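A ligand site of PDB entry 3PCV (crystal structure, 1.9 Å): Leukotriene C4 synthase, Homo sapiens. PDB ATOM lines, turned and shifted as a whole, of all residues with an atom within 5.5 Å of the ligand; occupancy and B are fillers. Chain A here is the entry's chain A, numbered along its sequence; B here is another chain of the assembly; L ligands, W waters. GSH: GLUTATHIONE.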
ATOM      1  N   ARG A  51       4.700   7.962  24.583  1.00  0.00           N
ATOM      2  CA  ARG A  51       5.942   8.339  25.217  1.00  0.00           C
ATOM      3  C   ARG A  51       6.538   7.159  26.008  1.00  0.00           C
ATOM      4  O   ARG A  51       7.781   7.023  26.057  1.00  0.00           O
ATOM      5  CB  ARG A  51       5.762   9.517  26.193  1.00  0.00           C
ATOM      6  CG  ARG A  51       5.633  10.922  25.508  1.00  0.00           C
ATOM      7  CD  ARG A  51       6.773  11.235  24.526  1.00  0.00           C
ATOM      8  NE  ARG A  51       8.094  10.980  25.112  1.00  0.00           N
ATOM      9  CZ  ARG A  51       9.200  10.886  24.392  1.00  0.00           C
ATOM     10  NH1 ARG A  51      10.353  10.573  24.985  1.00  0.00           N
ATOM     11  NH2 ARG A  51       9.134  11.059  23.067  1.00  0.00           N
ATOM     12  N   ALA A  52       5.683   6.368  26.671  1.00  0.00           N
ATOM     13  CA  ALA A  52       6.184   5.254  27.462  1.00  0.00           C
ATOM     14  C   ALA A  52       6.909   4.276  26.511  1.00  0.00           C
ATOM     15  O   ALA A  52       7.996   3.754  26.826  1.00  0.00           O
ATOM     16  CB  ALA A  52       5.049   4.553  28.204  1.00  0.00           C
ATOM     17  N   ASN A  55      10.256   5.864  25.237  1.00  0.00           N
ATOM     18  CA  ASN A  55      11.290   5.869  26.274  1.00  0.00           C
ATOM     19  C   ASN A  55      11.869   4.441  26.418  1.00  0.00           C
ATOM     20  O   ASN A  55      13.106   4.241  26.465  1.00  0.00           O
ATOM     21  CB  ASN A  55      10.686   6.309  27.637  1.00  0.00           C
ATOM     22  CG  ASN A  55      11.751   6.546  28.711  1.00  0.00           C
ATOM     23  OD1 ASN A  55      12.206   5.596  29.356  1.00  0.00           O
ATOM     24  ND2 ASN A  55      12.143   7.796  28.911  1.00  0.00           N
ATOM     25  N   GLU A  58      14.165   3.772  23.446  1.00  0.00           N
ATOM     26  CA  GLU A  58      15.473   4.403  23.368  1.00  0.00           C
ATOM     27  C   GLU A  58      16.473   3.845  24.386  1.00  0.00           C
ATOM     28  O   GLU A  58      17.678   3.903  24.117  1.00  0.00           O
ATOM     29  CB  GLU A  58      15.413   5.940  23.450  1.00  0.00           C
ATOM     30  CG  GLU A  58      14.975   6.421  24.765  1.00  0.00           C
ATOM     31  CD  GLU A  58      14.550   7.924  24.749  1.00  0.00           C
ATOM     32  OE1 GLU A  58      14.595   8.606  23.691  1.00  0.00           O
ATOM     33  OE2 GLU A  58      14.148   8.386  25.807  1.00  0.00           O
ATOM     34  N   TYR A  59      16.003   3.292  25.492  1.00  0.00           N
ATOM     35  CA  TYR A  59      16.924   2.609  26.426  1.00  0.00           C
ATOM     36  C   TYR A  59      17.222   1.154  26.033  1.00  0.00           C
ATOM     37  O   TYR A  59      18.174   0.546  26.540  1.00  0.00           O
ATOM     38  CB  TYR A  59      16.404   2.639  27.851  1.00  0.00           C
ATOM     39  CG  TYR A  59      16.524   4.005  28.470  1.00  0.00           C
ATOM     40  CD1 TYR A  59      17.651   4.375  29.189  1.00  0.00           C
ATOM     41  CD2 TYR A  59      15.505   4.946  28.296  1.00  0.00           C
ATOM     42  CE1 TYR A  59      17.773   5.645  29.751  1.00  0.00           C
ATOM     43  CE2 TYR A  59      15.614   6.243  28.842  1.00  0.00           C
ATOM     44  CZ  TYR A  59      16.725   6.578  29.586  1.00  0.00           C
ATOM     45  OH  TYR A  59      16.845   7.847  30.134  1.00  0.00           O
ATOM     46  N   TYR A  93       6.901   0.285  34.345  1.00  0.00           N
ATOM     47  CA  TYR A  93       7.049   1.667  33.917  1.00  0.00           C
ATOM     48  C   TYR A  93       6.027   1.985  32.826  1.00  0.00           C
ATOM     49  O   TYR A  93       5.405   3.062  32.861  1.00  0.00           O
ATOM     50  CB  TYR A  93       8.470   1.901  33.380  1.00  0.00           C
ATOM     51  CG  TYR A  93       8.704   3.214  32.647  1.00  0.00           C
ATOM     52  CD1 TYR A  93       9.122   4.333  33.339  1.00  0.00           C
ATOM     53  CD2 TYR A  93       8.518   3.322  31.278  1.00  0.00           C
ATOM     54  CE1 TYR A  93       9.345   5.546  32.692  1.00  0.00           C
ATOM     55  CE2 TYR A  93       8.771   4.542  30.607  1.00  0.00           C
ATOM     56  CZ  TYR A  93       9.161   5.632  31.332  1.00  0.00           C
ATOM     57  OH  TYR A  93       9.427   6.828  30.705  1.00  0.00           O
ATOM     58  N   TYR A  97       3.152   4.619  33.538  1.00  0.00           N
ATOM     59  CA  TYR A  97       3.146   5.822  32.734  1.00  0.00           C
ATOM     60  C   TYR A  97       1.831   5.950  31.958  1.00  0.00           C
ATOM     61  O   TYR A  97       1.250   7.048  31.861  1.00  0.00           O
ATOM     62  CB  TYR A  97       4.355   5.793  31.768  1.00  0.00           C
ATOM     63  CG  TYR A  97       4.796   7.104  31.144  1.00  0.00           C
ATOM     64  CD1 TYR A  97       4.053   8.295  31.262  1.00  0.00           C
ATOM     65  CD2 TYR A  97       5.963   7.145  30.388  1.00  0.00           C
ATOM     66  CE1 TYR A  97       4.471   9.472  30.657  1.00  0.00           C
ATOM     67  CE2 TYR A  97       6.403   8.310  29.796  1.00  0.00           C
ATOM     68  CZ  TYR A  97       5.651   9.487  29.930  1.00  0.00           C
ATOM     69  OH  TYR A  97       6.120  10.622  29.297  1.00  0.00           O
ATOM     70  N   ARG A 104       4.865   6.626  36.540  1.00  0.00           N
ATOM     71  CA  ARG A 104       6.093   6.114  35.845  1.00  0.00           C
ATOM     72  C   ARG A 104       7.320   6.113  36.765  1.00  0.00           C
ATOM     73  O   ARG A 104       8.292   5.385  36.492  1.00  0.00           O
ATOM     74  CB  ARG A 104       6.432   6.941  34.618  1.00  0.00           C
ATOM     75  CG  ARG A 104       7.321   8.174  34.899  1.00  0.00           C
ATOM     76  CD  ARG A 104       7.413   9.086  33.637  1.00  0.00           C
ATOM     77  NE  ARG A 104       8.356  10.191  33.882  1.00  0.00           N
ATOM     78  CZ  ARG A 104       8.098  11.250  34.645  1.00  0.00           C
ATOM     79  NH1 ARG A 104       9.035  12.171  34.799  1.00  0.00           N
ATOM     80  NH2 ARG A 104       6.903  11.387  35.240  1.00  0.00           N
ATOM     81  N   LEU A 105       7.294   6.903  37.841  1.00  0.00           N
ATOM     82  CA  LEU A 105       8.515   7.222  38.574  1.00  0.00           C
ATOM     83  C   LEU A 105       9.100   6.063  39.371  1.00  0.00           C
ATOM     84  O   LEU A 105      10.311   5.808  39.282  1.00  0.00           O
ATOM     85  CB  LEU A 105       8.367   8.475  39.478  1.00  0.00           C
ATOM     86  CG  LEU A 105       8.147   9.790  38.713  1.00  0.00           C
ATOM     87  CD1 LEU A 105       7.685  10.937  39.650  1.00  0.00           C
ATOM     88  CD2 LEU A 105       9.395  10.179  37.904  1.00  0.00           C
ATOM     89  N   LEU A 108      10.468   3.551  37.013  1.00  0.00           N
ATOM     90  CA  LEU A 108      11.635   4.132  36.350  1.00  0.00           C
ATOM     91  C   LEU A 108      12.886   4.016  37.235  1.00  0.00           C
ATOM     92  O   LEU A 108      13.986   3.691  36.752  1.00  0.00           O
ATOM     93  CB  LEU A 108      11.420   5.604  35.969  1.00  0.00           C
ATOM     94  CG  LEU A 108      12.644   6.321  35.377  1.00  0.00           C
ATOM     95  CD1 LEU A 108      13.066   5.716  34.024  1.00  0.00           C
ATOM     96  CD2 LEU A 108      12.381   7.830  35.231  1.00  0.00           C
ATOM     97  N   SER B  23      20.919  11.321  28.779  1.00  0.00           N
ATOM     98  CA  SER B  23      19.634  11.132  29.447  1.00  0.00           C
ATOM     99  C   SER B  23      19.537  11.976  30.722  1.00  0.00           C
ATOM    100  O   SER B  23      18.517  12.614  30.962  1.00  0.00           O
ATOM    101  CB  SER B  23      19.403   9.652  29.760  1.00  0.00           C
ATOM    102  OG  SER B  23      19.280   8.896  28.569  1.00  0.00           O
ATOM    103  N   VAL B  26      18.984  15.626  29.799  1.00  0.00           N
ATOM    104  CA  VAL B  26      17.575  15.908  29.443  1.00  0.00           C
ATOM    105  C   VAL B  26      16.711  16.029  30.717  1.00  0.00           C
ATOM    106  O   VAL B  26      15.830  16.911  30.795  1.00  0.00           O
ATOM    107  CB  VAL B  26      16.975  14.793  28.547  1.00  0.00           C
ATOM    108  CG1 VAL B  26      15.461  14.990  28.366  1.00  0.00           C
ATOM    109  CG2 VAL B  26      17.677  14.784  27.174  1.00  0.00           C
ATOM    110  N   ILE B  27      16.930  15.161  31.682  1.00  0.00           N
ATOM    111  CA  ILE B  27      16.150  15.208  32.950  1.00  0.00           C
ATOM    112  C   ILE B  27      16.426  16.554  33.653  1.00  0.00           C
ATOM    113  O   ILE B  27      15.499  17.222  34.135  1.00  0.00           O
ATOM    114  CB  ILE B  27      16.491  14.008  33.841  1.00  0.00           C
ATOM    115  CG1 ILE B  27      15.876  12.737  33.236  1.00  0.00           C
ATOM    116  CG2 ILE B  27      15.987  14.214  35.337  1.00  0.00           C
ATOM    117  CD1 ILE B  27      16.458  11.429  33.853  1.00  0.00           C
ATOM    118  N   ARG B  30      14.544  19.213  31.816  1.00  0.00           N
ATOM    119  CA  ARG B  30      13.122  19.132  32.127  1.00  0.00           C
ATOM    120  C   ARG B  30      12.820  19.888  33.427  1.00  0.00           C
ATOM    121  O   ARG B  30      11.828  20.617  33.531  1.00  0.00           O
ATOM    122  CB  ARG B  30      12.681  17.679  32.286  1.00  0.00           C
ATOM    123  CG  ARG B  30      12.457  16.956  30.948  1.00  0.00           C
ATOM    124  CD  ARG B  30      11.784  15.601  31.162  1.00  0.00           C
ATOM    125  NE  ARG B  30      11.540  14.938  29.878  1.00  0.00           N
ATOM    126  CZ  ARG B  30      10.516  15.236  29.087  1.00  0.00           C
ATOM    127  NH1 ARG B  30       9.649  16.182  29.444  1.00  0.00           N
ATOM    128  NH2 ARG B  30      10.350  14.594  27.945  1.00  0.00           N
ATOM    129  N   PRO B  37       6.912  15.332  31.500  1.00  0.00           N
ATOM    130  CA  PRO B  37       6.401  14.280  30.623  1.00  0.00           C
ATOM    131  C   PRO B  37       4.865  14.272  30.758  1.00  0.00           C
ATOM    132  O   PRO B  37       4.360  14.442  31.866  1.00  0.00           O
ATOM    133  CB  PRO B  37       6.972  12.995  31.260  1.00  0.00           C
ATOM    134  CG  PRO B  37       8.317  13.464  31.832  1.00  0.00           C
ATOM    135  CD  PRO B  37       7.992  14.846  32.402  1.00  0.00           C
ATOM    136  N   PRO B  38       4.142  13.996  29.668  1.00  0.00           N
ATOM    137  CA  PRO B  38       4.675  13.474  28.401  1.00  0.00           C
ATOM    138  C   PRO B  38       5.105  14.520  27.365  1.00  0.00           C
ATOM    139  O   PRO B  38       5.345  14.176  26.214  1.00  0.00           O
ATOM    140  CB  PRO B  38       3.510  12.640  27.855  1.00  0.00           C
ATOM    141  CG  PRO B  38       2.274  13.468  28.320  1.00  0.00           C
ATOM    142  CD  PRO B  38       2.665  13.914  29.720  1.00  0.00           C
ATOM    143  N   THR B  40       7.312  16.887  25.077  1.00  0.00           N
ATOM    144  CA  THR B  40       8.674  16.950  24.572  1.00  0.00           C
ATOM    145  C   THR B  40       8.865  18.281  23.818  1.00  0.00           C
ATOM    146  O   THR B  40       9.803  18.456  23.028  1.00  0.00           O
ATOM    147  CB  THR B  40       8.968  15.767  23.646  1.00  0.00           C
ATOM    148  OG1 THR B  40       7.965  15.749  22.609  1.00  0.00           O
ATOM    149  CG2 THR B  40       8.838  14.464  24.459  1.00  0.00           C
ATOM    150  N   TYR B  50      16.726  17.952  24.371  1.00  0.00           N
ATOM    151  CA  TYR B  50      15.894  16.794  24.096  1.00  0.00           C
ATOM    152  C   TYR B  50      16.266  16.186  22.745  1.00  0.00           C
ATOM    153  O   TYR B  50      16.550  14.966  22.647  1.00  0.00           O
ATOM    154  CB  TYR B  50      14.403  17.171  24.120  1.00  0.00           C
ATOM    155  CG  TYR B  50      13.520  16.087  23.556  1.00  0.00           C
ATOM    156  CD1 TYR B  50      13.179  14.977  24.330  1.00  0.00           C
ATOM    157  CD2 TYR B  50      13.070  16.150  22.255  1.00  0.00           C
ATOM    158  CE1 TYR B  50      12.375  13.965  23.806  1.00  0.00           C
ATOM    159  CE2 TYR B  50      12.275  15.145  21.724  1.00  0.00           C
ATOM    160  CZ  TYR B  50      11.954  14.050  22.509  1.00  0.00           C
ATOM    161  OH  TYR B  50      11.199  13.039  21.968  1.00  0.00           O
ATOM    162  N   GLN B  53      19.763  14.537  22.511  1.00  0.00           N
ATOM    163  CA  GLN B  53      19.724  13.189  23.116  1.00  0.00           C
ATOM    164  C   GLN B  53      19.037  12.174  22.196  1.00  0.00           C
ATOM    165  O   GLN B  53      19.549  11.062  21.970  1.00  0.00           O
ATOM    166  CB  GLN B  53      19.082  13.217  24.513  1.00  0.00           C
ATOM    167  CG  GLN B  53      18.829  11.790  25.164  1.00  0.00           C
ATOM    168  CD  GLN B  53      17.412  11.273  24.863  1.00  0.00           C
ATOM    169  OE1 GLN B  53      16.431  11.895  25.244  1.00  0.00           O
ATOM    170  NE2 GLN B  53      17.307  10.129  24.169  1.00  0.00           N
ATOM    171  N   VAL B  54      17.892  12.554  21.632  1.00  0.00           N
ATOM    172  CA  VAL B  54      17.163  11.647  20.756  1.00  0.00           C
ATOM    173  C   VAL B  54      17.991  11.285  19.517  1.00  0.00           C
ATOM    174  O   VAL B  54      18.012  10.110  19.075  1.00  0.00           O
ATOM    175  CB  VAL B  54      15.802  12.271  20.292  1.00  0.00           C
ATOM    176  CG1 VAL B  54      15.162  11.446  19.134  1.00  0.00           C
ATOM    177  CG2 VAL B  54      14.843  12.373  21.480  1.00  0.00           C
HETATM  178  N1  GSH L   1      13.916  10.960  26.201  1.00  0.00           N
HETATM  179  CA1 GSH L   1      13.796  11.050  27.664  1.00  0.00           C
HETATM  180  C1  GSH L   1      12.945  12.274  28.020  1.00  0.00           C
HETATM  181  O11 GSH L   1      12.717  12.605  29.186  1.00  0.00           O
HETATM  182  O12 GSH L   1      12.466  13.020  27.136  1.00  0.00           O
HETATM  183  CB1 GSH L   1      15.212  11.128  28.276  1.00  0.00           C
HETATM  184  CG1 GSH L   1      15.301  11.361  29.802  1.00  0.00           C
HETATM  185  CD1 GSH L   1      14.411  10.408  30.593  1.00  0.00           C
HETATM  186  OE1 GSH L   1      14.528   9.030  30.417  1.00  0.00           O
HETATM  187  N2  GSH L   1      13.513  10.928  31.447  1.00  0.00           N
HETATM  188  CA2 GSH L   1      12.669  10.124  32.295  1.00  0.00           C
HETATM  189  C2  GSH L   1      11.348   9.859  31.606  1.00  0.00           C
HETATM  190  O2  GSH L   1      10.419   9.044  32.190  1.00  0.00           O
HETATM  191  CB2 GSH L   1      12.442  10.838  33.643  1.00  0.00           C
HETATM  192  SG2 GSH L   1      11.857  12.526  33.274  1.00  0.00           S
HETATM  193  N3  GSH L   1      11.042  10.424  30.457  1.00  0.00           N
HETATM  194  CA3 GSH L   1       9.652  10.460  30.033  1.00  0.00           C
HETATM  195  C3  GSH L   1       9.547  10.362  28.519  1.00  0.00           C
HETATM  196  O31 GSH L   1      10.565  10.053  27.834  1.00  0.00           O
HETATM  197  O32 GSH L   1       8.442  10.559  27.953  1.00  0.00           O
HETATM  198  O   HOH W   1      12.757  10.573  23.567  1.00  0.00           O
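CD2 of Leu 108 touches CB2 of the ligand, 3.4 Å away. Ser 23 of chain B touches the ligand (O to CG1, 3.6 Å). Val 26 of chain B touches the ligand. Ile 27 of chain B touches the ligand (CG1 to N2, 3.5 Å). Pro 37 of chain B touches the ligand (CG to CA3, 3.7 Å). Tyr 50 of chain B touches the ligand (CE1 to O12, 3.5 Å). 15 residues have an atom within 4 Å of the ligand: Arg 51, Asn 55, Glu 58, Tyr 59, Tyr 93, Tyr 97, Arg 104, Leu 108, Ser 23 of chain B, Val 26 of chain B, Ile 27 of chain B, Arg 30 of chain B, Pro 37 of chain B, Tyr 50 of chain B and Gln 53 of chain B.
Water W1 lies within hydrogen-bond range of the side-chain carboxylate (OE1) of Glu 58 (2.7 Å), the guanidinium group (NH1) of Arg 51 (2.8 Å), a nitrogen (N1) of the ligand (2.9 Å) and the side-chain hydroxyl (OH) of Tyr 50 of chain B (3.3 Å).
The side-chain hydroxyl (OG) of Ser 23 of chain B sits at hydrogen-bond distance from the side-chain hydroxyl (OH) of Tyr 59 (3.1 Å). OH of Tyr 93 sits close to OD1 of Asn 55 (3.3 Å). The side-chain amide nitrogen (NE2) of Gln 53 of chain B is in hydrogen-bond range of the side-chain carboxylate (OE1) of Glu 58 (3.1 Å). The guanidinium group of Arg 51 is in hydrogen-bond range of the side-chain hydroxyl of Tyr 50 of chain B (3.1 Å).
An oxygen (O32) of the ligand lies within hydrogen-bond range of the side-chain hydroxyl (OH) of Tyr 97 (2.7 Å). The guanidinium group of Arg 51 is in salt-bridge range of an oxygen (O32) of the ligand (2.9 Å). The guanidinium group (NE) of Arg 30 of chain B is in salt-bridge range of an oxygen (O11) of the ligand. A nitrogen (N1) of the ligand lies within salt-bridge range of the side-chain carboxylate (OE2) of Glu 58, 2.6 Å away. The side-chain hydroxyl of Tyr 93 is in hydrogen-bond range of an oxygen (O2) of the ligand, 2.8 Å away. OE1 of Gln 53 of chain B is in hydrogen-bond range of N1 of the ligand (2.8 Å). The side-chain amide nitrogen (ND2) of Asn 55 sits at hydrogen-bond distance from an oxygen (O31) of the ligand, 3.0 Å away. The guanidinium group (NE) of Arg 104 lies within hydrogen-bond range of an oxygen (O2) of the ligand (2.9 Å). The side-chain hydroxyl (OH) of Tyr 59 sits at hydrogen-bond distance from an oxygen (OE1) of the ligand, 2.6 Å away.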
